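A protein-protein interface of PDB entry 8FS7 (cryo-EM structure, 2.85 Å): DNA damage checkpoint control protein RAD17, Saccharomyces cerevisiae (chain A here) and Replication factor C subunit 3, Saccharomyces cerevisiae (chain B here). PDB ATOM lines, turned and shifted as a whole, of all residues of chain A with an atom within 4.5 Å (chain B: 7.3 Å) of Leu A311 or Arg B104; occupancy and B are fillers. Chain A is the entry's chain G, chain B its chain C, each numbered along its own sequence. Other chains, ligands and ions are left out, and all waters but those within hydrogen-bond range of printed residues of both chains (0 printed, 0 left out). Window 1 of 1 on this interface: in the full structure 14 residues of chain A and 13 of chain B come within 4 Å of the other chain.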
ATOM      1  N   HIS A  54      20.024  23.217  12.767  1.00  0.00           N
ATOM      2  CA  HIS A  54      19.610  23.118  11.366  1.00  0.00           C
ATOM      3  C   HIS A  54      19.941  24.373  10.561  1.00  0.00           C
ATOM      4  O   HIS A  54      19.312  24.634   9.531  1.00  0.00           O
ATOM      5  CB  HIS A  54      18.114  22.798  11.244  1.00  0.00           C
ATOM      6  CG  HIS A  54      17.691  21.581  12.005  1.00  0.00           C
ATOM      7  ND1 HIS A  54      16.879  21.644  13.117  1.00  0.00           N
ATOM      8  CD2 HIS A  54      17.965  20.269  11.813  1.00  0.00           C
ATOM      9  CE1 HIS A  54      16.671  20.424  13.577  1.00  0.00           C
ATOM     10  NE2 HIS A  54      17.319  19.571  12.805  1.00  0.00           N
ATOM     11  N   VAL A  55      20.916  25.161  11.007  1.00  0.00           N
ATOM     12  CA  VAL A  55      21.313  26.364  10.291  1.00  0.00           C
ATOM     13  C   VAL A  55      22.765  26.337   9.835  1.00  0.00           C
ATOM     14  O   VAL A  55      23.122  27.090   8.914  1.00  0.00           O
ATOM     15  CB  VAL A  55      21.047  27.630  11.134  1.00  0.00           C
ATOM     16  CG1 VAL A  55      19.567  27.756  11.455  1.00  0.00           C
ATOM     17  CG2 VAL A  55      21.876  27.609  12.409  1.00  0.00           C
ATOM     18  N   LEU A 145      21.704  20.990   4.444  1.00  0.00           N
ATOM     19  CA  LEU A 145      22.292  22.302   4.176  1.00  0.00           C
ATOM     20  C   LEU A 145      23.327  22.149   3.065  1.00  0.00           C
ATOM     21  O   LEU A 145      24.532  22.020   3.297  1.00  0.00           O
ATOM     22  CB  LEU A 145      22.907  22.885   5.443  1.00  0.00           C
ATOM     23  CG  LEU A 145      21.964  23.115   6.624  1.00  0.00           C
ATOM     24  CD1 LEU A 145      22.745  23.206   7.922  1.00  0.00           C
ATOM     25  CD2 LEU A 145      21.144  24.374   6.409  1.00  0.00           C
ATOM     26  N   PHE A 237      24.601  37.424   7.764  1.00  0.00           N
ATOM     27  CA  PHE A 237      24.836  36.202   8.516  1.00  0.00           C
ATOM     28  C   PHE A 237      24.976  36.520   9.995  1.00  0.00           C
ATOM     29  O   PHE A 237      25.591  37.522  10.370  1.00  0.00           O
ATOM     30  CB  PHE A 237      26.096  35.480   8.024  1.00  0.00           C
ATOM     31  CG  PHE A 237      26.040  35.084   6.580  1.00  0.00           C
ATOM     32  CD1 PHE A 237      25.308  33.980   6.180  1.00  0.00           C
ATOM     33  CD2 PHE A 237      26.718  35.817   5.621  1.00  0.00           C
ATOM     34  CE1 PHE A 237      25.254  33.613   4.851  1.00  0.00           C
ATOM     35  CE2 PHE A 237      26.667  35.455   4.291  1.00  0.00           C
ATOM     36  CZ  PHE A 237      25.934  34.352   3.905  1.00  0.00           C
ATOM     37  N   VAL A 261      21.752  32.462  -4.480  1.00  0.00           N
ATOM     38  CA  VAL A 261      20.680  33.409  -4.174  1.00  0.00           C
ATOM     39  C   VAL A 261      19.732  32.899  -3.104  1.00  0.00           C
ATOM     40  O   VAL A 261      18.919  33.679  -2.590  1.00  0.00           O
ATOM     41  CB  VAL A 261      19.840  33.756  -5.421  1.00  0.00           C
ATOM     42  CG1 VAL A 261      20.533  34.815  -6.263  1.00  0.00           C
ATOM     43  CG2 VAL A 261      19.570  32.510  -6.235  1.00  0.00           C
ATOM     44  N   GLY A 263      20.418  32.140  -0.141  1.00  0.00           N
ATOM     45  CA  GLY A 263      20.927  32.453   1.182  1.00  0.00           C
ATOM     46  C   GLY A 263      21.647  31.317   1.877  1.00  0.00           C
ATOM     47  O   GLY A 263      21.415  31.079   3.068  1.00  0.00           O
ATOM     48  N   VAL A 264      22.511  30.603   1.161  1.00  0.00           N
ATOM     49  CA  VAL A 264      23.322  29.534   1.732  1.00  0.00           C
ATOM     50  C   VAL A 264      24.781  29.842   1.428  1.00  0.00           C
ATOM     51  O   VAL A 264      25.152  30.025   0.263  1.00  0.00           O
ATOM     52  CB  VAL A 264      22.926  28.155   1.180  1.00  0.00           C
ATOM     53  CG1 VAL A 264      23.917  27.096   1.636  1.00  0.00           C
ATOM     54  CG2 VAL A 264      21.515  27.792   1.618  1.00  0.00           C
ATOM     55  N   CYS A 309      28.698  24.722   5.675  1.00  0.00           N
ATOM     56  CA  CYS A 309      27.539  25.330   5.041  1.00  0.00           C
ATOM     57  C   CYS A 309      26.761  26.134   6.074  1.00  0.00           C
ATOM     58  O   CYS A 309      26.510  25.655   7.184  1.00  0.00           O
ATOM     59  CB  CYS A 309      26.639  24.271   4.404  1.00  0.00           C
ATOM     60  SG  CYS A 309      27.338  23.514   2.918  1.00  0.00           S
ATOM     61  N   MET A 310      26.382  27.355   5.706  1.00  0.00           N
ATOM     62  CA  MET A 310      25.775  28.282   6.649  1.00  0.00           C
ATOM     63  C   MET A 310      24.595  28.981   5.986  1.00  0.00           C
ATOM     64  O   MET A 310      24.657  29.355   4.812  1.00  0.00           O
ATOM     65  CB  MET A 310      26.805  29.306   7.145  1.00  0.00           C
ATOM     66  CG  MET A 310      26.228  30.498   7.893  1.00  0.00           C
ATOM     67  SD  MET A 310      27.482  31.622   8.546  1.00  0.00           S
ATOM     68  CE  MET A 310      28.999  30.793   8.075  1.00  0.00           C
ATOM     69  N   LEU A 311      23.520  29.149   6.751  1.00  0.00           N
ATOM     70  CA  LEU A 311      22.322  29.833   6.293  1.00  0.00           C
ATOM     71  C   LEU A 311      22.455  31.341   6.478  1.00  0.00           C
ATOM     72  O   LEU A 311      23.240  31.827   7.296  1.00  0.00           O
ATOM     73  CB  LEU A 311      21.086  29.323   7.040  1.00  0.00           C
ATOM     74  CG  LEU A 311      20.422  28.061   6.489  1.00  0.00           C
ATOM     75  CD1 LEU A 311      19.265  27.634   7.378  1.00  0.00           C
ATOM     76  CD2 LEU A 311      19.951  28.282   5.060  1.00  0.00           C
ATOM     77  N   GLU A 312      21.665  32.078   5.704  1.00  0.00           N
ATOM     78  CA  GLU A 312      21.666  33.532   5.716  1.00  0.00           C
ATOM     79  C   GLU A 312      20.452  34.053   6.479  1.00  0.00           C
ATOM     80  O   GLU A 312      19.355  33.498   6.386  1.00  0.00           O
ATOM     81  CB  GLU A 312      21.672  34.078   4.286  1.00  0.00           C
ATOM     82  CG  GLU A 312      21.358  35.558   4.144  1.00  0.00           C
ATOM     83  CD  GLU A 312      21.909  36.150   2.862  1.00  0.00           C
ATOM     84  OE1 GLU A 312      22.634  35.434   2.140  1.00  0.00           O
ATOM     85  OE2 GLU A 312      21.617  37.330   2.577  1.00  0.00           O
ATOM     86  N   LYS A 313      20.665  35.123   7.243  1.00  0.00           N
ATOM     87  CA  LYS A 313      19.587  35.742   7.999  1.00  0.00           C
ATOM     88  C   LYS A 313      18.532  36.322   7.059  1.00  0.00           C
ATOM     89  O   LYS A 313      18.813  36.694   5.915  1.00  0.00           O
ATOM     90  CB  LYS A 313      20.134  36.838   8.912  1.00  0.00           C
ATOM     91  CG  LYS A 313      21.125  36.346   9.954  1.00  0.00           C
ATOM     92  CD  LYS A 313      20.424  35.972  11.249  1.00  0.00           C
ATOM     93  CE  LYS A 313      19.840  37.199  11.929  1.00  0.00           C
ATOM     94  NZ  LYS A 313      20.876  38.238  12.188  1.00  0.00           N
ATOM     95  N   GLU A 314      17.296  36.386   7.560  1.00  0.00           N
ATOM     96  CA  GLU A 314      16.178  36.834   6.734  1.00  0.00           C
ATOM     97  C   GLU A 314      16.321  38.300   6.340  1.00  0.00           C
ATOM     98  O   GLU A 314      16.007  38.671   5.202  1.00  0.00           O
ATOM     99  CB  GLU A 314      14.857  36.595   7.471  1.00  0.00           C
ATOM    100  CG  GLU A 314      13.685  37.464   7.011  1.00  0.00           C
ATOM    101  CD  GLU A 314      13.056  37.015   5.696  1.00  0.00           C
ATOM    102  OE1 GLU A 314      11.849  37.276   5.507  1.00  0.00           O
ATOM    103  OE2 GLU A 314      13.747  36.403   4.854  1.00  0.00           O
ATOM    104  N   ASN B  77      14.873  19.532   8.004  1.00  0.00           N
ATOM    105  CA  ASN B  77      15.375  20.885   8.213  1.00  0.00           C
ATOM    106  C   ASN B  77      14.289  21.951   8.181  1.00  0.00           C
ATOM    107  O   ASN B  77      14.541  23.081   8.615  1.00  0.00           O
ATOM    108  CB  ASN B  77      16.451  21.214   7.171  1.00  0.00           C
ATOM    109  CG  ASN B  77      16.192  20.550   5.834  1.00  0.00           C
ATOM    110  OD1 ASN B  77      15.044  20.359   5.436  1.00  0.00           O
ATOM    111  ND2 ASN B  77      17.261  20.194   5.134  1.00  0.00           N
ATOM    112  N   MET B  78      13.096  21.633   7.685  1.00  0.00           N
ATOM    113  CA  MET B  78      11.989  22.581   7.666  1.00  0.00           C
ATOM    114  C   MET B  78      11.121  22.500   8.913  1.00  0.00           C
ATOM    115  O   MET B  78      10.239  23.345   9.093  1.00  0.00           O
ATOM    116  CB  MET B  78      11.119  22.356   6.427  1.00  0.00           C
ATOM    117  CG  MET B  78      11.714  22.886   5.135  1.00  0.00           C
ATOM    118  SD  MET B  78      12.260  24.595   5.273  1.00  0.00           S
ATOM    119  CE  MET B  78      11.008  25.408   4.285  1.00  0.00           C
ATOM    120  N   ASP B  99      17.405  31.377  16.347  1.00  0.00           N
ATOM    121  CA  ASP B  99      18.311  31.049  15.252  1.00  0.00           C
ATOM    122  C   ASP B  99      17.599  30.252  14.167  1.00  0.00           C
ATOM    123  O   ASP B  99      17.843  30.461  12.974  1.00  0.00           O
ATOM    124  CB  ASP B  99      19.521  30.279  15.780  1.00  0.00           C
ATOM    125  CG  ASP B  99      20.466  31.155  16.578  1.00  0.00           C
ATOM    126  OD1 ASP B  99      20.147  32.347  16.779  1.00  0.00           O
ATOM    127  OD2 ASP B  99      21.527  30.654  17.003  1.00  0.00           O
ATOM    128  N   PHE B 100      16.722  29.326  14.562  1.00  0.00           N
ATOM    129  CA  PHE B 100      15.961  28.576  13.568  1.00  0.00           C
ATOM    130  C   PHE B 100      14.988  29.483  12.824  1.00  0.00           C
ATOM    131  O   PHE B 100      14.954  29.492  11.589  1.00  0.00           O
ATOM    132  CB  PHE B 100      15.218  27.417  14.231  1.00  0.00           C
ATOM    133  CG  PHE B 100      14.489  26.533  13.258  1.00  0.00           C
ATOM    134  CD1 PHE B 100      15.179  25.599  12.503  1.00  0.00           C
ATOM    135  CD2 PHE B 100      13.120  26.644  13.089  1.00  0.00           C
ATOM    136  CE1 PHE B 100      14.514  24.786  11.604  1.00  0.00           C
ATOM    137  CE2 PHE B 100      12.450  25.836  12.191  1.00  0.00           C
ATOM    138  CZ  PHE B 100      13.147  24.905  11.448  1.00  0.00           C
ATOM    139  N   ALA B 101      14.188  30.255  13.557  1.00  0.00           N
ATOM    140  CA  ALA B 101      13.266  31.210  12.944  1.00  0.00           C
ATOM    141  C   ALA B 101      13.893  32.594  12.824  1.00  0.00           C
ATOM    142  O   ALA B 101      13.305  33.605  13.202  1.00  0.00           O
ATOM    143  CB  ALA B 101      11.972  31.265  13.746  1.00  0.00           C
ATOM    144  N   SER B 102      15.110  32.640  12.290  1.00  0.00           N
ATOM    145  CA  SER B 102      15.735  33.883  11.863  1.00  0.00           C
ATOM    146  C   SER B 102      16.441  33.777  10.521  1.00  0.00           C
ATOM    147  O   SER B 102      16.706  34.815   9.905  1.00  0.00           O
ATOM    148  CB  SER B 102      16.742  34.376  12.913  1.00  0.00           C
ATOM    149  OG  SER B 102      16.086  34.761  14.108  1.00  0.00           O
ATOM    150  N   THR B 103      16.754  32.574  10.051  1.00  0.00           N
ATOM    151  CA  THR B 103      17.417  32.378   8.774  1.00  0.00           C
ATOM    152  C   THR B 103      16.393  32.133   7.670  1.00  0.00           C
ATOM    153  O   THR B 103      15.230  31.813   7.923  1.00  0.00           O
ATOM    154  CB  THR B 103      18.396  31.208   8.846  1.00  0.00           C
ATOM    155  OG1 THR B 103      17.698  30.023   9.250  1.00  0.00           O
ATOM    156  CG2 THR B 103      19.502  31.501   9.849  1.00  0.00           C
ATOM    157  N   ARG B 104      16.849  32.287   6.430  1.00  0.00           N
ATOM    158  CA  ARG B 104      15.988  32.086   5.277  1.00  0.00           C
ATOM    159  C   ARG B 104      15.754  30.594   5.037  1.00  0.00           C
ATOM    160  O   ARG B 104      16.450  29.728   5.576  1.00  0.00           O
ATOM    161  CB  ARG B 104      16.600  32.733   4.036  1.00  0.00           C
ATOM    162  CG  ARG B 104      17.014  34.181   4.233  1.00  0.00           C
ATOM    163  CD  ARG B 104      16.876  34.978   2.950  1.00  0.00           C
ATOM    164  NE  ARG B 104      18.156  35.132   2.269  1.00  0.00           N
ATOM    165  CZ  ARG B 104      18.307  35.688   1.074  1.00  0.00           C
ATOM    166  NH1 ARG B 104      17.274  36.157   0.394  1.00  0.00           N
ATOM    167  NH2 ARG B 104      19.526  35.774   0.549  1.00  0.00           N
ATOM    168  N   GLN B 105      14.748  30.301   4.217  1.00  0.00           N
ATOM    169  CA  GLN B 105      14.460  28.924   3.841  1.00  0.00           C
ATOM    170  C   GLN B 105      15.575  28.379   2.955  1.00  0.00           C
ATOM    171  O   GLN B 105      16.253  29.127   2.246  1.00  0.00           O
ATOM    172  CB  GLN B 105      13.119  28.841   3.110  1.00  0.00           C
ATOM    173  CG  GLN B 105      12.058  29.793   3.646  1.00  0.00           C
ATOM    174  CD  GLN B 105      11.795  29.611   5.128  1.00  0.00           C
ATOM    175  OE1 GLN B 105      11.734  30.582   5.881  1.00  0.00           O
ATOM    176  NE2 GLN B 105      11.634  28.366   5.554  1.00  0.00           N
ATOM    177  N   ILE B 106      15.767  27.061   3.001  1.00  0.00           N
ATOM    178  CA  ILE B 106      16.890  26.458   2.291  1.00  0.00           C
ATOM    179  C   ILE B 106      16.617  26.473   0.794  1.00  0.00           C
ATOM    180  O   ILE B 106      17.275  27.200   0.042  1.00  0.00           O
ATOM    181  CB  ILE B 106      17.150  25.023   2.785  1.00  0.00           C
ATOM    182  CG1 ILE B 106      17.117  24.971   4.316  1.00  0.00           C
ATOM    183  CG2 ILE B 106      18.477  24.508   2.241  1.00  0.00           C
ATOM    184  CD1 ILE B 106      17.847  23.787   4.915  1.00  0.00           C
ATOM    185  N   PHE B 107      15.644  25.679   0.347  1.00  0.00           N
ATOM    186  CA  PHE B 107      15.142  25.820  -1.014  1.00  0.00           C
ATOM    187  C   PHE B 107      13.647  25.556  -1.132  1.00  0.00           C
ATOM    188  O   PHE B 107      13.099  25.712  -2.227  1.00  0.00           O
ATOM    189  CB  PHE B 107      15.932  24.882  -1.956  1.00  0.00           C
ATOM    190  CG  PHE B 107      15.588  25.044  -3.412  1.00  0.00           C
ATOM    191  CD1 PHE B 107      15.685  26.281  -4.025  1.00  0.00           C
ATOM    192  CD2 PHE B 107      15.153  23.962  -4.160  1.00  0.00           C
ATOM    193  CE1 PHE B 107      15.362  26.437  -5.358  1.00  0.00           C
ATOM    194  CE2 PHE B 107      14.829  24.111  -5.496  1.00  0.00           C
ATOM    195  CZ  PHE B 107      14.933  25.350  -6.095  1.00  0.00           C
ATOM    196  N   LYS B 112       8.878  28.034   7.621  1.00  0.00           N
ATOM    197  CA  LYS B 112       9.463  27.116   8.588  1.00  0.00           C
ATOM    198  C   LYS B 112       8.424  26.769   9.645  1.00  0.00           C
ATOM    199  O   LYS B 112       7.649  27.628  10.073  1.00  0.00           O
ATOM    200  CB  LYS B 112      10.702  27.725   9.245  1.00  0.00           C
ATOM    201  CG  LYS B 112      12.018  27.222   8.676  1.00  0.00           C
ATOM    202  CD  LYS B 112      13.163  28.164   9.009  1.00  0.00           C
ATOM    203  CE  LYS B 112      14.472  27.673   8.413  1.00  0.00           C
ATOM    204  NZ  LYS B 112      15.618  27.867   9.345  1.00  0.00           N
ATOM    205  N   ASN B 140       8.008  34.187   7.689  1.00  0.00           N
ATOM    206  CA  ASN B 140       8.608  32.970   7.164  1.00  0.00           C
ATOM    207  C   ASN B 140       8.553  31.792   8.126  1.00  0.00           C
ATOM    208  O   ASN B 140       9.087  30.725   7.801  1.00  0.00           O
ATOM    209  CB  ASN B 140      10.067  33.233   6.763  1.00  0.00           C
ATOM    210  CG  ASN B 140      10.874  33.877   7.878  1.00  0.00           C
ATOM    211  OD1 ASN B 140      10.969  33.346   8.985  1.00  0.00           O
ATOM    212  ND2 ASN B 140      11.457  35.033   7.589  1.00  0.00           N
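Hydrophobic or aromatic side chains of chain A within 4 Å of the printed part of chain B: Val A55, Leu A145 and Leu A311. Among the printed residues, 14 pairs touch across the chains. Among the printed residues, Asp or Glu carboxylates within 4 Å of a Lys or Arg side-chain nitrogen of the other chain: Glu A312 with Arg B104.
Of the printed residues of chain B, Leu A311 touches Thr B103 (3.4 Å) and Arg B104 (3.8 Å). Arg B104 touches six residues of chain A. Of the printed residues of chain A, Ser B102 touches Lys A313 (3.6 Å) and Glu A314 (2.9 Å). Printed residues of chain A within 4 Å of Asp B99: Val A55 (3.5 Å). Printed residues of chain B within 4 Å of Val A55: Asp B99 (3.5 Å) and Thr B103 (3.7 Å). Of the printed residues of chain B, Glu A314 touches Ser B102 (2.9 Å), Arg B104 (3.7 Å) and Asn B140 (3.1 Å). Phe A237 touches none of the printed residues of chain B. Met B78 touches none of the printed residues of chain A. The nearest printed residue of chain B that does not touch Val A261 is Ile B106 (7.0 Å).
O of Ser B102 sits at hydrogen-bond distance from N of Glu A314, 2.9 Å away. The guanidinium group (NH2) of Arg B104 lies within salt-bridge range of the side-chain carboxylate (OE2) of Glu A312, 3.3 Å away. The side-chain carboxylate of Glu A314 is in hydrogen-bond range of the side-chain amide nitrogen of Asn B140 (3.1 Å).
Among the printed residues, pairs that only touch across the chains: Val A55 with Asp B99 (3.5 Å), Val A55 with Thr B103 (3.7 Å), Leu A145 with Ile B106 (3.7 Å), Val A261 with Arg B104 (3.8 Å), Gly A263 with Arg B104 (3.7 Å), Leu A311 with Thr B103 (3.4 Å), Leu A311 with Arg B104 (3.8 Å), Glu A312 with Thr B103 (3.3 Å), Lys A313 with Ser B102 (3.6 Å), Lys A313 with Arg B104 (3.5 Å) and Glu A314 with Arg B104 (3.7 Å).
OG1 of Thr B103 lies within hydrogen-bond range of NZ of Lys B112 (3.0 Å). OE1 of Gln B105 lies close to O of Asn B140 (3.3 Å). The backbone NH of Lys B112 is in hydrogen-bond range of the backbone carbonyl oxygen of Asn B140 (2.7 Å). O of Val A55 is in hydrogen-bond range of N of Leu A311. O of Leu A145 lies within hydrogen-bond range of SG of Cys A309, at 3.2 Å. The backbone NH (N) of Glu A312 sits at hydrogen-bond distance from the backbone carbonyl oxygen (O) of Gly A263 (2.8 Å).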
